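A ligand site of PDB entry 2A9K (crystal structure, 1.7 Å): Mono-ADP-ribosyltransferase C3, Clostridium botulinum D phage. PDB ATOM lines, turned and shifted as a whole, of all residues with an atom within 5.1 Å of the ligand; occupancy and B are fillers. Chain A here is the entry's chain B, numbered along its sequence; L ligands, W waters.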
ATOM      1  N   TYR A  51      23.718  17.447 -15.765  1.00  0.00           N
ATOM      2  CA  TYR A  51      23.691  18.431 -16.843  1.00  0.00           C
ATOM      3  C   TYR A  51      25.090  18.991 -17.134  1.00  0.00           C
ATOM      4  O   TYR A  51      25.487  19.083 -18.297  1.00  0.00           O
ATOM      5  CB  TYR A  51      22.693  19.574 -16.593  1.00  0.00           C
ATOM      6  CG  TYR A  51      22.842  20.672 -17.616  1.00  0.00           C
ATOM      7  CD1 TYR A  51      22.132  20.639 -18.818  1.00  0.00           C
ATOM      8  CD2 TYR A  51      23.727  21.725 -17.399  1.00  0.00           C
ATOM      9  CE1 TYR A  51      22.288  21.652 -19.774  1.00  0.00           C
ATOM     10  CE2 TYR A  51      23.904  22.730 -18.353  1.00  0.00           C
ATOM     11  CZ  TYR A  51      23.167  22.679 -19.531  1.00  0.00           C
ATOM     12  OH  TYR A  51      23.329  23.659 -20.471  1.00  0.00           O
ATOM     13  N   THR A  52      25.830  19.363 -16.090  1.00  0.00           N
ATOM     14  CA  THR A  52      27.163  19.968 -16.283  1.00  0.00           C
ATOM     15  C   THR A  52      28.152  19.008 -16.945  1.00  0.00           C
ATOM     16  O   THR A  52      29.099  19.447 -17.606  1.00  0.00           O
ATOM     17  CB  THR A  52      27.749  20.569 -14.977  1.00  0.00           C
ATOM     18  OG1 THR A  52      27.854  19.551 -13.959  1.00  0.00           O
ATOM     19  CG2 THR A  52      26.894  21.720 -14.477  1.00  0.00           C
ATOM     20  N   LYS A  53      27.899  17.707 -16.802  1.00  0.00           N
ATOM     21  CA  LYS A  53      28.698  16.648 -17.447  1.00  0.00           C
ATOM     22  C   LYS A  53      28.240  16.297 -18.865  1.00  0.00           C
ATOM     23  O   LYS A  53      28.994  15.692 -19.638  1.00  0.00           O
ATOM     24  CB  LYS A  53      28.665  15.365 -16.591  1.00  0.00           C
ATOM     25  CG  LYS A  53      29.289  15.486 -15.209  1.00  0.00           C
ATOM     26  CD  LYS A  53      29.134  14.181 -14.429  1.00  0.00           C
ATOM     27  CE  LYS A  53      29.458  14.371 -12.957  1.00  0.00           C
ATOM     28  NZ  LYS A  53      29.074  13.194 -12.126  1.00  0.00           N
ATOM     29  N   ALA A  55      25.812  18.426 -20.965  1.00  0.00           N
ATOM     30  CA  ALA A  55      25.024  19.515 -21.541  1.00  0.00           C
ATOM     31  C   ALA A  55      24.846  19.442 -23.058  1.00  0.00           C
ATOM     32  O   ALA A  55      23.719  19.488 -23.548  1.00  0.00           O
ATOM     33  CB  ALA A  55      25.637  20.847 -21.153  1.00  0.00           C
ATOM     34  N   SER A  56      25.949  19.329 -23.790  1.00  0.00           N
ATOM     35  CA  SER A  56      25.900  19.316 -25.264  1.00  0.00           C
ATOM     36  C   SER A  56      25.042  18.166 -25.831  1.00  0.00           C
ATOM     37  O   SER A  56      24.462  18.317 -26.906  1.00  0.00           O
ATOM     38  CB  SER A  56      27.306  19.289 -25.851  1.00  0.00           C
ATOM     39  OG  SER A  56      27.963  18.064 -25.540  1.00  0.00           O
ATOM     40  N   ASN A  59      21.227  19.213 -24.692  1.00  0.00           N
ATOM     41  CA  ASN A  59      20.884  20.372 -25.528  1.00  0.00           C
ATOM     42  C   ASN A  59      20.825  20.004 -27.008  1.00  0.00           C
ATOM     43  O   ASN A  59      20.001  20.557 -27.753  1.00  0.00           O
ATOM     44  CB  ASN A  59      21.862  21.514 -25.289  1.00  0.00           C
ATOM     45  CG  ASN A  59      21.815  22.061 -23.868  1.00  0.00           C
ATOM     46  OD1 ASN A  59      20.773  22.028 -23.214  1.00  0.00           O
ATOM     47  ND2 ASN A  59      22.942  22.572 -23.396  1.00  0.00           N
ATOM     48  N   ARG A  63      17.625  20.602 -29.362  1.00  0.00           N
ATOM     49  CA  ARG A  63      17.758  21.323 -30.617  1.00  0.00           C
ATOM     50  C   ARG A  63      17.300  20.481 -31.813  1.00  0.00           C
ATOM     51  O   ARG A  63      16.619  21.007 -32.697  1.00  0.00           O
ATOM     52  CB  ARG A  63      19.195  21.817 -30.833  1.00  0.00           C
ATOM     53  CG  ARG A  63      19.555  23.020 -29.972  1.00  0.00           C
ATOM     54  CD  ARG A  63      20.893  23.639 -30.366  1.00  0.00           C
ATOM     55  NE  ARG A  63      22.030  22.951 -29.758  1.00  0.00           N
ATOM     56  CZ  ARG A  63      22.550  23.232 -28.561  1.00  0.00           C
ATOM     57  NH1 ARG A  63      22.031  24.190 -27.808  1.00  0.00           N
ATOM     58  NH2 ARG A  63      23.580  22.533 -28.116  1.00  0.00           N
ATOM     59  N   PHE A  99      27.591  36.020 -19.282  1.00  0.00           N
ATOM     60  CA  PHE A  99      28.509  35.849 -20.393  1.00  0.00           C
ATOM     61  C   PHE A  99      28.504  34.429 -20.922  1.00  0.00           C
ATOM     62  O   PHE A  99      28.471  33.471 -20.145  1.00  0.00           O
ATOM     63  CB  PHE A  99      29.929  36.238 -19.973  1.00  0.00           C
ATOM     64  CG  PHE A  99      30.069  37.690 -19.636  1.00  0.00           C
ATOM     65  CD1 PHE A  99      29.818  38.129 -18.338  1.00  0.00           C
ATOM     66  CD2 PHE A  99      30.452  38.604 -20.602  1.00  0.00           C
ATOM     67  CE1 PHE A  99      29.958  39.484 -18.018  1.00  0.00           C
ATOM     68  CE2 PHE A  99      30.583  39.948 -20.288  1.00  0.00           C
ATOM     69  CZ  PHE A  99      30.333  40.388 -18.989  1.00  0.00           C
ATOM     70  N   ARG A 100      28.581  34.297 -22.235  1.00  0.00           N
ATOM     71  CA  ARG A 100      28.532  33.008 -22.883  1.00  0.00           C
ATOM     72  C   ARG A 100      29.486  32.949 -24.068  1.00  0.00           C
ATOM     73  O   ARG A 100      29.575  33.902 -24.849  1.00  0.00           O
ATOM     74  CB  ARG A 100      27.090  32.714 -23.304  1.00  0.00           C
ATOM     75  CG  ARG A 100      26.999  31.709 -24.402  1.00  0.00           C
ATOM     76  CD  ARG A 100      25.790  30.845 -24.316  1.00  0.00           C
ATOM     77  NE  ARG A 100      25.985  29.730 -25.232  1.00  0.00           N
ATOM     78  CZ  ARG A 100      26.075  28.453 -24.860  1.00  0.00           C
ATOM     79  NH1 ARG A 100      25.953  28.104 -23.597  1.00  0.00           N
ATOM     80  NH2 ARG A 100      26.267  27.533 -25.798  1.00  0.00           N
ATOM     81  N   GLY A 101      30.213  31.833 -24.185  1.00  0.00           N
ATOM     82  CA  GLY A 101      31.055  31.563 -25.349  1.00  0.00           C
ATOM     83  C   GLY A 101      30.430  30.557 -26.303  1.00  0.00           C
ATOM     84  O   GLY A 101      29.886  29.533 -25.872  1.00  0.00           O
ATOM     85  N   ASP A 102      30.515  30.843 -27.597  1.00  0.00           N
ATOM     86  CA  ASP A 102      29.970  29.963 -28.626  1.00  0.00           C
ATOM     87  C   ASP A 102      30.921  29.707 -29.775  1.00  0.00           C
ATOM     88  O   ASP A 102      31.722  30.570 -30.152  1.00  0.00           O
ATOM     89  CB  ASP A 102      28.637  30.506 -29.168  1.00  0.00           C
ATOM     90  CG  ASP A 102      27.450  30.085 -28.329  1.00  0.00           C
ATOM     91  OD1 ASP A 102      27.060  28.891 -28.384  1.00  0.00           O
ATOM     92  OD2 ASP A 102      26.886  30.948 -27.622  1.00  0.00           O
ATOM     93  N   ASP A 103      30.807  28.512 -30.352  1.00  0.00           N
ATOM     94  CA  ASP A 103      31.538  28.116 -31.549  1.00  0.00           C
ATOM     95  C   ASP A 103      30.737  28.481 -32.789  1.00  0.00           C
ATOM     96  O   ASP A 103      29.543  28.770 -32.682  1.00  0.00           O
ATOM     97  CB  ASP A 103      31.828  26.612 -31.480  1.00  0.00           C
ATOM     98  CG  ASP A 103      32.735  26.250 -30.322  1.00  0.00           C
ATOM     99  OD1 ASP A 103      33.878  26.730 -30.302  1.00  0.00           O
ATOM    100  OD2 ASP A 103      32.278  25.497 -29.431  1.00  0.00           O
ATOM    101  N   ALA A 105      29.159  27.082 -35.260  1.00  0.00           N
ATOM    102  CA  ALA A 105      27.879  26.430 -35.582  1.00  0.00           C
ATOM    103  C   ALA A 105      26.656  27.067 -34.905  1.00  0.00           C
ATOM    104  O   ALA A 105      25.516  26.864 -35.354  1.00  0.00           O
ATOM    105  CB  ALA A 105      27.941  24.936 -35.275  1.00  0.00           C
ATOM    106  N   TYR A 106      26.898  27.838 -33.851  1.00  0.00           N
ATOM    107  CA  TYR A 106      25.854  28.642 -33.214  1.00  0.00           C
ATOM    108  C   TYR A 106      25.167  29.630 -34.192  1.00  0.00           C
ATOM    109  O   TYR A 106      23.987  29.957 -34.027  1.00  0.00           O
ATOM    110  CB  TYR A 106      26.409  29.382 -31.966  1.00  0.00           C
ATOM    111  CG  TYR A 106      25.510  30.494 -31.451  1.00  0.00           C
ATOM    112  CD1 TYR A 106      24.466  30.225 -30.560  1.00  0.00           C
ATOM    113  CD2 TYR A 106      25.703  31.801 -31.873  1.00  0.00           C
ATOM    114  CE1 TYR A 106      23.635  31.264 -30.106  1.00  0.00           C
ATOM    115  CE2 TYR A 106      24.885  32.835 -31.429  1.00  0.00           C
ATOM    116  CZ  TYR A 106      23.854  32.560 -30.549  1.00  0.00           C
ATOM    117  OH  TYR A 106      23.056  33.589 -30.128  1.00  0.00           O
ATOM    118  N   ARG A 139      15.575  35.547 -31.042  1.00  0.00           N
ATOM    119  CA  ARG A 139      16.130  34.231 -31.261  1.00  0.00           C
ATOM    120  C   ARG A 139      15.648  33.291 -30.179  1.00  0.00           C
ATOM    121  O   ARG A 139      15.673  33.637 -29.001  1.00  0.00           O
ATOM    122  CB  ARG A 139      17.666  34.274 -31.298  1.00  0.00           C
ATOM    123  CG  ARG A 139      18.284  32.902 -31.405  1.00  0.00           C
ATOM    124  CD  ARG A 139      19.735  32.922 -31.840  1.00  0.00           C
ATOM    125  NE  ARG A 139      20.245  31.556 -31.881  1.00  0.00           N
ATOM    126  CZ  ARG A 139      21.319  31.152 -32.560  1.00  0.00           C
ATOM    127  NH1 ARG A 139      22.034  32.019 -33.269  1.00  0.00           N
ATOM    128  NH2 ARG A 139      21.677  29.878 -32.539  1.00  0.00           N
ATOM    129  N   GLU A 141      16.150  29.648 -28.303  1.00  0.00           N
ATOM    130  CA  GLU A 141      17.101  28.588 -28.001  1.00  0.00           C
ATOM    131  C   GLU A 141      16.364  27.396 -27.380  1.00  0.00           C
ATOM    132  O   GLU A 141      15.745  27.540 -26.325  1.00  0.00           O
ATOM    133  CB  GLU A 141      18.203  29.106 -27.076  1.00  0.00           C
ATOM    134  CG  GLU A 141      19.289  28.070 -26.723  1.00  0.00           C
ATOM    135  CD  GLU A 141      19.846  27.359 -27.962  1.00  0.00           C
ATOM    136  OE1 GLU A 141      20.279  28.046 -28.918  1.00  0.00           O
ATOM    137  OE2 GLU A 141      19.847  26.098 -27.961  1.00  0.00           O
ATOM    138  N   TYR A 144      18.985  24.338 -22.888  1.00  0.00           N
ATOM    139  CA  TYR A 144      19.291  25.177 -21.718  1.00  0.00           C
ATOM    140  C   TYR A 144      20.474  26.041 -22.108  1.00  0.00           C
ATOM    141  O   TYR A 144      21.256  25.662 -22.980  1.00  0.00           O
ATOM    142  CB  TYR A 144      19.638  24.329 -20.489  1.00  0.00           C
ATOM    143  CG  TYR A 144      18.535  23.375 -20.085  1.00  0.00           C
ATOM    144  CD1 TYR A 144      17.529  23.781 -19.200  1.00  0.00           C
ATOM    145  CD2 TYR A 144      18.468  22.083 -20.616  1.00  0.00           C
ATOM    146  CE1 TYR A 144      16.492  22.909 -18.835  1.00  0.00           C
ATOM    147  CE2 TYR A 144      17.431  21.211 -20.251  1.00  0.00           C
ATOM    148  CZ  TYR A 144      16.454  21.632 -19.366  1.00  0.00           C
ATOM    149  OH  TYR A 144      15.437  20.773 -19.022  1.00  0.00           O
ATOM    150  N   SER A 146      23.855  27.684 -20.787  1.00  0.00           N
ATOM    151  CA  SER A 146      24.915  27.811 -19.801  1.00  0.00           C
ATOM    152  C   SER A 146      25.640  29.124 -20.007  1.00  0.00           C
ATOM    153  O   SER A 146      26.056  29.448 -21.123  1.00  0.00           O
ATOM    154  CB  SER A 146      25.902  26.638 -19.909  1.00  0.00           C
ATOM    155  OG  SER A 146      25.287  25.425 -19.508  1.00  0.00           O
ATOM    156  N   THR A 147      25.755  29.897 -18.927  1.00  0.00           N
ATOM    157  CA  THR A 147      26.470  31.178 -18.967  1.00  0.00           C
ATOM    158  C   THR A 147      27.393  31.273 -17.744  1.00  0.00           C
ATOM    159  O   THR A 147      27.340  30.426 -16.864  1.00  0.00           O
ATOM    160  CB  THR A 147      25.500  32.377 -18.943  1.00  0.00           C
ATOM    161  OG1 THR A 147      24.955  32.539 -17.623  1.00  0.00           O
ATOM    162  CG2 THR A 147      24.371  32.225 -19.964  1.00  0.00           C
ATOM    163  N   SER A 148      28.212  32.320 -17.709  1.00  0.00           N
ATOM    164  CA  SER A 148      29.063  32.598 -16.550  1.00  0.00           C
ATOM    165  C   SER A 148      28.811  34.008 -16.019  1.00  0.00           C
ATOM    166  O   SER A 148      28.421  34.897 -16.777  1.00  0.00           O
ATOM    167  CB  SER A 148      30.534  32.427 -16.922  1.00  0.00           C
ATOM    168  OG  SER A 148      31.387  32.688 -15.811  1.00  0.00           O
ATOM    169  N   PHE A 155      35.558  29.485 -21.743  1.00  0.00           N
ATOM    170  CA  PHE A 155      34.673  29.731 -22.877  1.00  0.00           C
ATOM    171  C   PHE A 155      34.861  31.140 -23.443  1.00  0.00           C
ATOM    172  O   PHE A 155      34.369  31.454 -24.523  1.00  0.00           O
ATOM    173  CB  PHE A 155      33.212  29.482 -22.469  1.00  0.00           C
ATOM    174  CG  PHE A 155      33.002  28.123 -21.870  1.00  0.00           C
ATOM    175  CD1 PHE A 155      32.901  26.999 -22.678  1.00  0.00           C
ATOM    176  CD2 PHE A 155      32.933  27.965 -20.486  1.00  0.00           C
ATOM    177  CE1 PHE A 155      32.721  25.726 -22.127  1.00  0.00           C
ATOM    178  CE2 PHE A 155      32.761  26.702 -19.931  1.00  0.00           C
ATOM    179  CZ  PHE A 155      32.659  25.586 -20.753  1.00  0.00           C
ATOM    180  N   ARG A 158      36.282  31.372 -27.037  1.00  0.00           N
ATOM    181  CA  ARG A 158      35.526  30.943 -28.219  1.00  0.00           C
ATOM    182  C   ARG A 158      35.332  32.134 -29.169  1.00  0.00           C
ATOM    183  O   ARG A 158      35.459  33.283 -28.741  1.00  0.00           O
ATOM    184  CB  ARG A 158      34.226  30.232 -27.816  1.00  0.00           C
ATOM    185  CG  ARG A 158      34.445  29.205 -26.705  1.00  0.00           C
ATOM    186  CD  ARG A 158      33.828  27.849 -26.955  1.00  0.00           C
ATOM    187  NE  ARG A 158      32.402  27.820 -26.643  1.00  0.00           N
ATOM    188  CZ  ARG A 158      31.736  26.751 -26.197  1.00  0.00           C
ATOM    189  NH1 ARG A 158      32.360  25.592 -25.974  1.00  0.00           N
ATOM    190  NH2 ARG A 158      30.445  26.840 -25.974  1.00  0.00           N
ATOM    191  N   SER A 179      28.300  22.096  -9.578  1.00  0.00           N
ATOM    192  CA  SER A 179      28.781  21.756 -10.922  1.00  0.00           C
ATOM    193  C   SER A 179      29.942  20.765 -10.874  1.00  0.00           C
ATOM    194  O   SER A 179      30.756  20.784  -9.938  1.00  0.00           O
ATOM    195  CB  SER A 179      29.236  23.018 -11.648  1.00  0.00           C
ATOM    196  OG  SER A 179      29.826  22.718 -12.912  1.00  0.00           O
ATOM    197  N   PHE A 181      32.212  21.108 -12.791  1.00  0.00           N
ATOM    198  CA  PHE A 181      33.299  22.013 -13.168  1.00  0.00           C
ATOM    199  C   PHE A 181      33.206  23.331 -12.381  1.00  0.00           C
ATOM    200  O   PHE A 181      32.900  24.381 -12.949  1.00  0.00           O
ATOM    201  CB  PHE A 181      33.294  22.282 -14.680  1.00  0.00           C
ATOM    202  CG  PHE A 181      33.317  21.035 -15.518  1.00  0.00           C
ATOM    203  CD1 PHE A 181      34.516  20.375 -15.783  1.00  0.00           C
ATOM    204  CD2 PHE A 181      32.128  20.505 -16.028  1.00  0.00           C
ATOM    205  CE1 PHE A 181      34.542  19.201 -16.557  1.00  0.00           C
ATOM    206  CE2 PHE A 181      32.148  19.343 -16.797  1.00  0.00           C
ATOM    207  CZ  PHE A 181      33.355  18.689 -17.066  1.00  0.00           C
ATOM    208  N   GLN A 184      33.792  27.837 -13.023  1.00  0.00           N
ATOM    209  CA  GLN A 184      33.202  28.420 -14.221  1.00  0.00           C
ATOM    210  C   GLN A 184      32.217  29.558 -13.902  1.00  0.00           C
ATOM    211  O   GLN A 184      31.783  30.288 -14.798  1.00  0.00           O
ATOM    212  CB  GLN A 184      32.516  27.334 -15.069  1.00  0.00           C
ATOM    213  CG  GLN A 184      33.492  26.412 -15.828  1.00  0.00           C
ATOM    214  CD  GLN A 184      32.799  25.264 -16.552  1.00  0.00           C
ATOM    215  OE1 GLN A 184      31.618  24.989 -16.334  1.00  0.00           O
ATOM    216  NE2 GLN A 184      33.546  24.571 -17.415  1.00  0.00           N
ATOM    217  N   GLU A 186      29.111  29.323 -13.109  1.00  0.00           N
ATOM    218  CA  GLU A 186      27.985  29.056 -14.014  1.00  0.00           C
ATOM    219  C   GLU A 186      26.613  29.520 -13.535  1.00  0.00           C
ATOM    220  O   GLU A 186      26.188  29.186 -12.425  1.00  0.00           O
ATOM    221  CB  GLU A 186      27.907  27.588 -14.441  1.00  0.00           C
ATOM    222  CG  GLU A 186      26.766  27.366 -15.458  1.00  0.00           C
ATOM    223  CD  GLU A 186      26.696  25.968 -16.024  1.00  0.00           C
ATOM    224  OE1 GLU A 186      27.584  25.141 -15.722  1.00  0.00           O
ATOM    225  OE2 GLU A 186      25.751  25.712 -16.809  1.00  0.00           O
HETATM  226  P1  LIG L   1      25.833  23.822 -25.567  1.00  0.00           P
HETATM  227  O1  LIG L   1      25.093  25.084 -25.308  1.00  0.00           O
HETATM  228  O2  LIG L   1      24.937  22.649 -25.572  1.00  0.00           O
HETATM  229  O3  LIG L   1      26.580  23.933 -26.985  1.00  0.00           O
HETATM  230  C1  LIG L   1      27.314  22.861 -27.535  1.00  0.00           C
HETATM  231  C2  LIG L   1      27.900  23.329 -28.872  1.00  0.00           C
HETATM  232  O4  LIG L   1      26.865  23.751 -29.739  1.00  0.00           O
HETATM  233  C3  LIG L   1      28.817  24.536 -28.727  1.00  0.00           C
HETATM  234  O5  LIG L   1      29.806  24.437 -29.726  1.00  0.00           O
HETATM  235  C4  LIG L   1      27.890  25.706 -29.000  1.00  0.00           C
HETATM  236  O6  LIG L   1      28.549  26.875 -29.440  1.00  0.00           O
HETATM  237  C5  LIG L   1      26.959  25.126 -30.037  1.00  0.00           C
HETATM  238  N1  LIG L   1      25.606  25.733 -30.032  1.00  0.00           N
HETATM  239  C6  LIG L   1      24.984  26.420 -29.022  1.00  0.00           C
HETATM  240  N2  LIG L   1      23.756  26.788 -29.452  1.00  0.00           N
HETATM  241  C7  LIG L   1      23.581  26.331 -30.712  1.00  0.00           C
HETATM  242  C8  LIG L   1      22.522  26.419 -31.606  1.00  0.00           C
HETATM  243  N3  LIG L   1      21.398  27.052 -31.268  1.00  0.00           N
HETATM  244  N4  LIG L   1      22.646  25.826 -32.854  1.00  0.00           N
HETATM  245  C9  LIG L   1      23.801  25.158 -33.212  1.00  0.00           C
HETATM  246  N5  LIG L   1      24.855  25.080 -32.312  1.00  0.00           N
HETATM  247  C10 LIG L   1      24.742  25.659 -31.091  1.00  0.00           C
HETATM  248  O7  LIG L   1      27.019  23.543 -24.543  1.00  0.00           O
HETATM  249  P2  LIG L   1      28.231  24.557 -24.220  1.00  0.00           P
HETATM  250  O8  LIG L   1      27.705  25.783 -23.595  1.00  0.00           O
HETATM  251  O9  LIG L   1      29.135  24.675 -25.389  1.00  0.00           O
HETATM  252  O10 LIG L   1      28.951  23.672 -23.107  1.00  0.00           O
HETATM  253  C11 LIG L   1      28.202  23.262 -21.986  1.00  0.00           C
HETATM  254  C12 LIG L   1      29.179  22.856 -20.894  1.00  0.00           C
HETATM  255  O11 LIG L   1      29.992  23.957 -20.557  1.00  0.00           O
HETATM  256  C13 LIG L   1      28.436  22.463 -19.634  1.00  0.00           C
HETATM  257  O12 LIG L   1      29.211  21.464 -19.025  1.00  0.00           O
HETATM  258  C14 LIG L   1      28.428  23.726 -18.795  1.00  0.00           C
HETATM  259  O13 LIG L   1      28.525  23.417 -17.432  1.00  0.00           O
HETATM  260  C15 LIG L   1      29.652  24.497 -19.300  1.00  0.00           C
HETATM  261  N6  LIG L   1      29.465  25.973 -19.402  1.00  0.00           N
HETATM  262  C16 LIG L   1      29.580  26.615 -20.624  1.00  0.00           C
HETATM  263  C17 LIG L   1      29.430  27.999 -20.716  1.00  0.00           C
HETATM  264  C18 LIG L   1      29.634  28.706 -22.040  1.00  0.00           C
HETATM  265  O14 LIG L   1      29.955  30.071 -22.089  1.00  0.00           O
HETATM  266  N7  LIG L   1      29.512  28.024 -23.178  1.00  0.00           N
HETATM  267  C19 LIG L   1      29.158  28.728 -19.567  1.00  0.00           C
HETATM  268  C20 LIG L   1      29.036  28.085 -18.331  1.00  0.00           C
HETATM  269  C21 LIG L   1      29.198  26.703 -18.265  1.00  0.00           C
HETATM  270  O   HOH W   1      18.215  26.186 -30.477  1.00  0.00           O
HETATM  271  O   HOH W   2      22.966  28.111 -27.086  1.00  0.00           O
HETATM  272  O   HOH W   3      24.099  25.565 -22.592  1.00  0.00           O
HETATM  273  O   HOH W   4      22.416  25.984 -25.455  1.00  0.00           O
HETATM  274  O   HOH W   5      26.490  22.886 -32.849  1.00  0.00           O
HETATM  275  O   HOH W   6      21.317  26.202 -35.205  1.00  0.00           O
HETATM  276  O   HOH W   7      29.569  23.137 -32.229  1.00  0.00           O
HETATM  277  O   HOH W   8      32.531  22.075 -19.018  1.00  0.00           O
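O of Thr 52 is in hydrogen-bond range of O12 of the ligand (2.5 Å).
An oxygen (O9) of the ligand lies within salt-bridge range of the guanidinium group (NH2) of Arg 158 (2.6 Å).
The side-chain carboxylate (OE1) of Glu 186 is in hydrogen-bond range of an oxygen (O13) of the ligand, 2.6 Å away.
The backbone NH of Asp 103 sits at hydrogen-bond distance from an oxygen (O6) of the ligand (2.9 Å).
O5 of the ligand sits at hydrogen-bond distance from OD2 of Asp 103.
O6 of the ligand lies within hydrogen-bond range of OD1 of Asp 102 (2.7 Å).
N of Gly 101 sits at hydrogen-bond distance from O14 of the ligand (2.8 Å).
N7 of the ligand is in hydrogen-bond range of O of Gly 101 (3.1 Å).
The guanidinium group of Arg 100 is in salt-bridge range of an oxygen (O1) of the ligand (2.8 Å).
A nitrogen (N3) of the ligand is in hydrogen-bond range of the side-chain carboxylate (OE1) of Glu 141.
O2 of the ligand is in salt-bridge range of NH2 of Arg 63 (2.9 Å).
The side-chain amide nitrogen (ND2) of Asn 59 sits at hydrogen-bond distance from an oxygen (O2) of the ligand (3.0 Å).
The side-chain carboxylate of Asp 103 lies within salt-bridge range of the guanidinium group of Arg 158, 3.5 Å away.
NH2 of Arg 158 is in hydrogen-bond range of O of Gly 101 (2.8 Å).
The side-chain carboxylate (OE2) of Glu 186 is in hydrogen-bond range of the side-chain hydroxyl (OG) of Ser 146.
The guanidinium group of Arg 100 lies within salt-bridge range of the side-chain carboxylate of Asp 102 (2.8 Å).
The backbone carbonyl oxygen (O) of Ser 146 sits at hydrogen-bond distance from the guanidinium group (NH1) of Arg 100 (2.8 Å).
The side-chain amide nitrogen (ND2) of Asn 59 is in hydrogen-bond range of the backbone carbonyl oxygen (O) of Ala 55 (3.2 Å).
ND2 of Asn 59 sits at hydrogen-bond distance from OH of Tyr 51 (3.1 Å).
N of Tyr 144 sits at hydrogen-bond distance from OD1 of Asn 59 (2.9 Å).
The guanidinium group (NH2) of Arg 139 sits close to a nitrogen (N3) of the ligand (3.1 Å).
Merely in contact with the ligand: Phe 155 (3.1 Å), Ala 105 (3.2 Å), Thr 147 (3.2 Å), Ser 56 (3.5 Å), Gln 184 (3.5 Å), Ser 146 (3.5 Å), Ala 55 (3.6 Å) and Tyr 106 (3.7 Å).
Within 4 Å of the ligand: Thr 52, Ala 55, Ser 56, Asn 59, Arg 63, Arg 100, Gly 101, Asp 102, Asp 103, Ala 105, Tyr 106, Arg 139, Glu 141, Ser 146, Thr 147, Phe 155, Arg 158, Gln 184 and Glu 186.
The nearest printed residue that does not touch the ligand is Ser 148 (4.2 Å).
Water W2 lies within hydrogen-bond range of a nitrogen (N2) of the ligand and the side-chain carboxylate (OE1) of Glu 141.
Water W4 lies within hydrogen-bond range of the backbone carbonyl oxygen (O) of Tyr 144 (2.8 Å), an oxygen (O1) of the ligand (2.8 Å) and the guanidinium group (NH1) of Arg 63 (3.0 Å).
Water W8 bridges the side-chain amide nitrogen of Gln 184 (3.1 Å) and an oxygen (O12) of the ligand (3.4 Å).
Water W1 lies within hydrogen-bond range of OE2 of Glu 141 (3.0 Å) and N3 of the ligand (3.4 Å).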
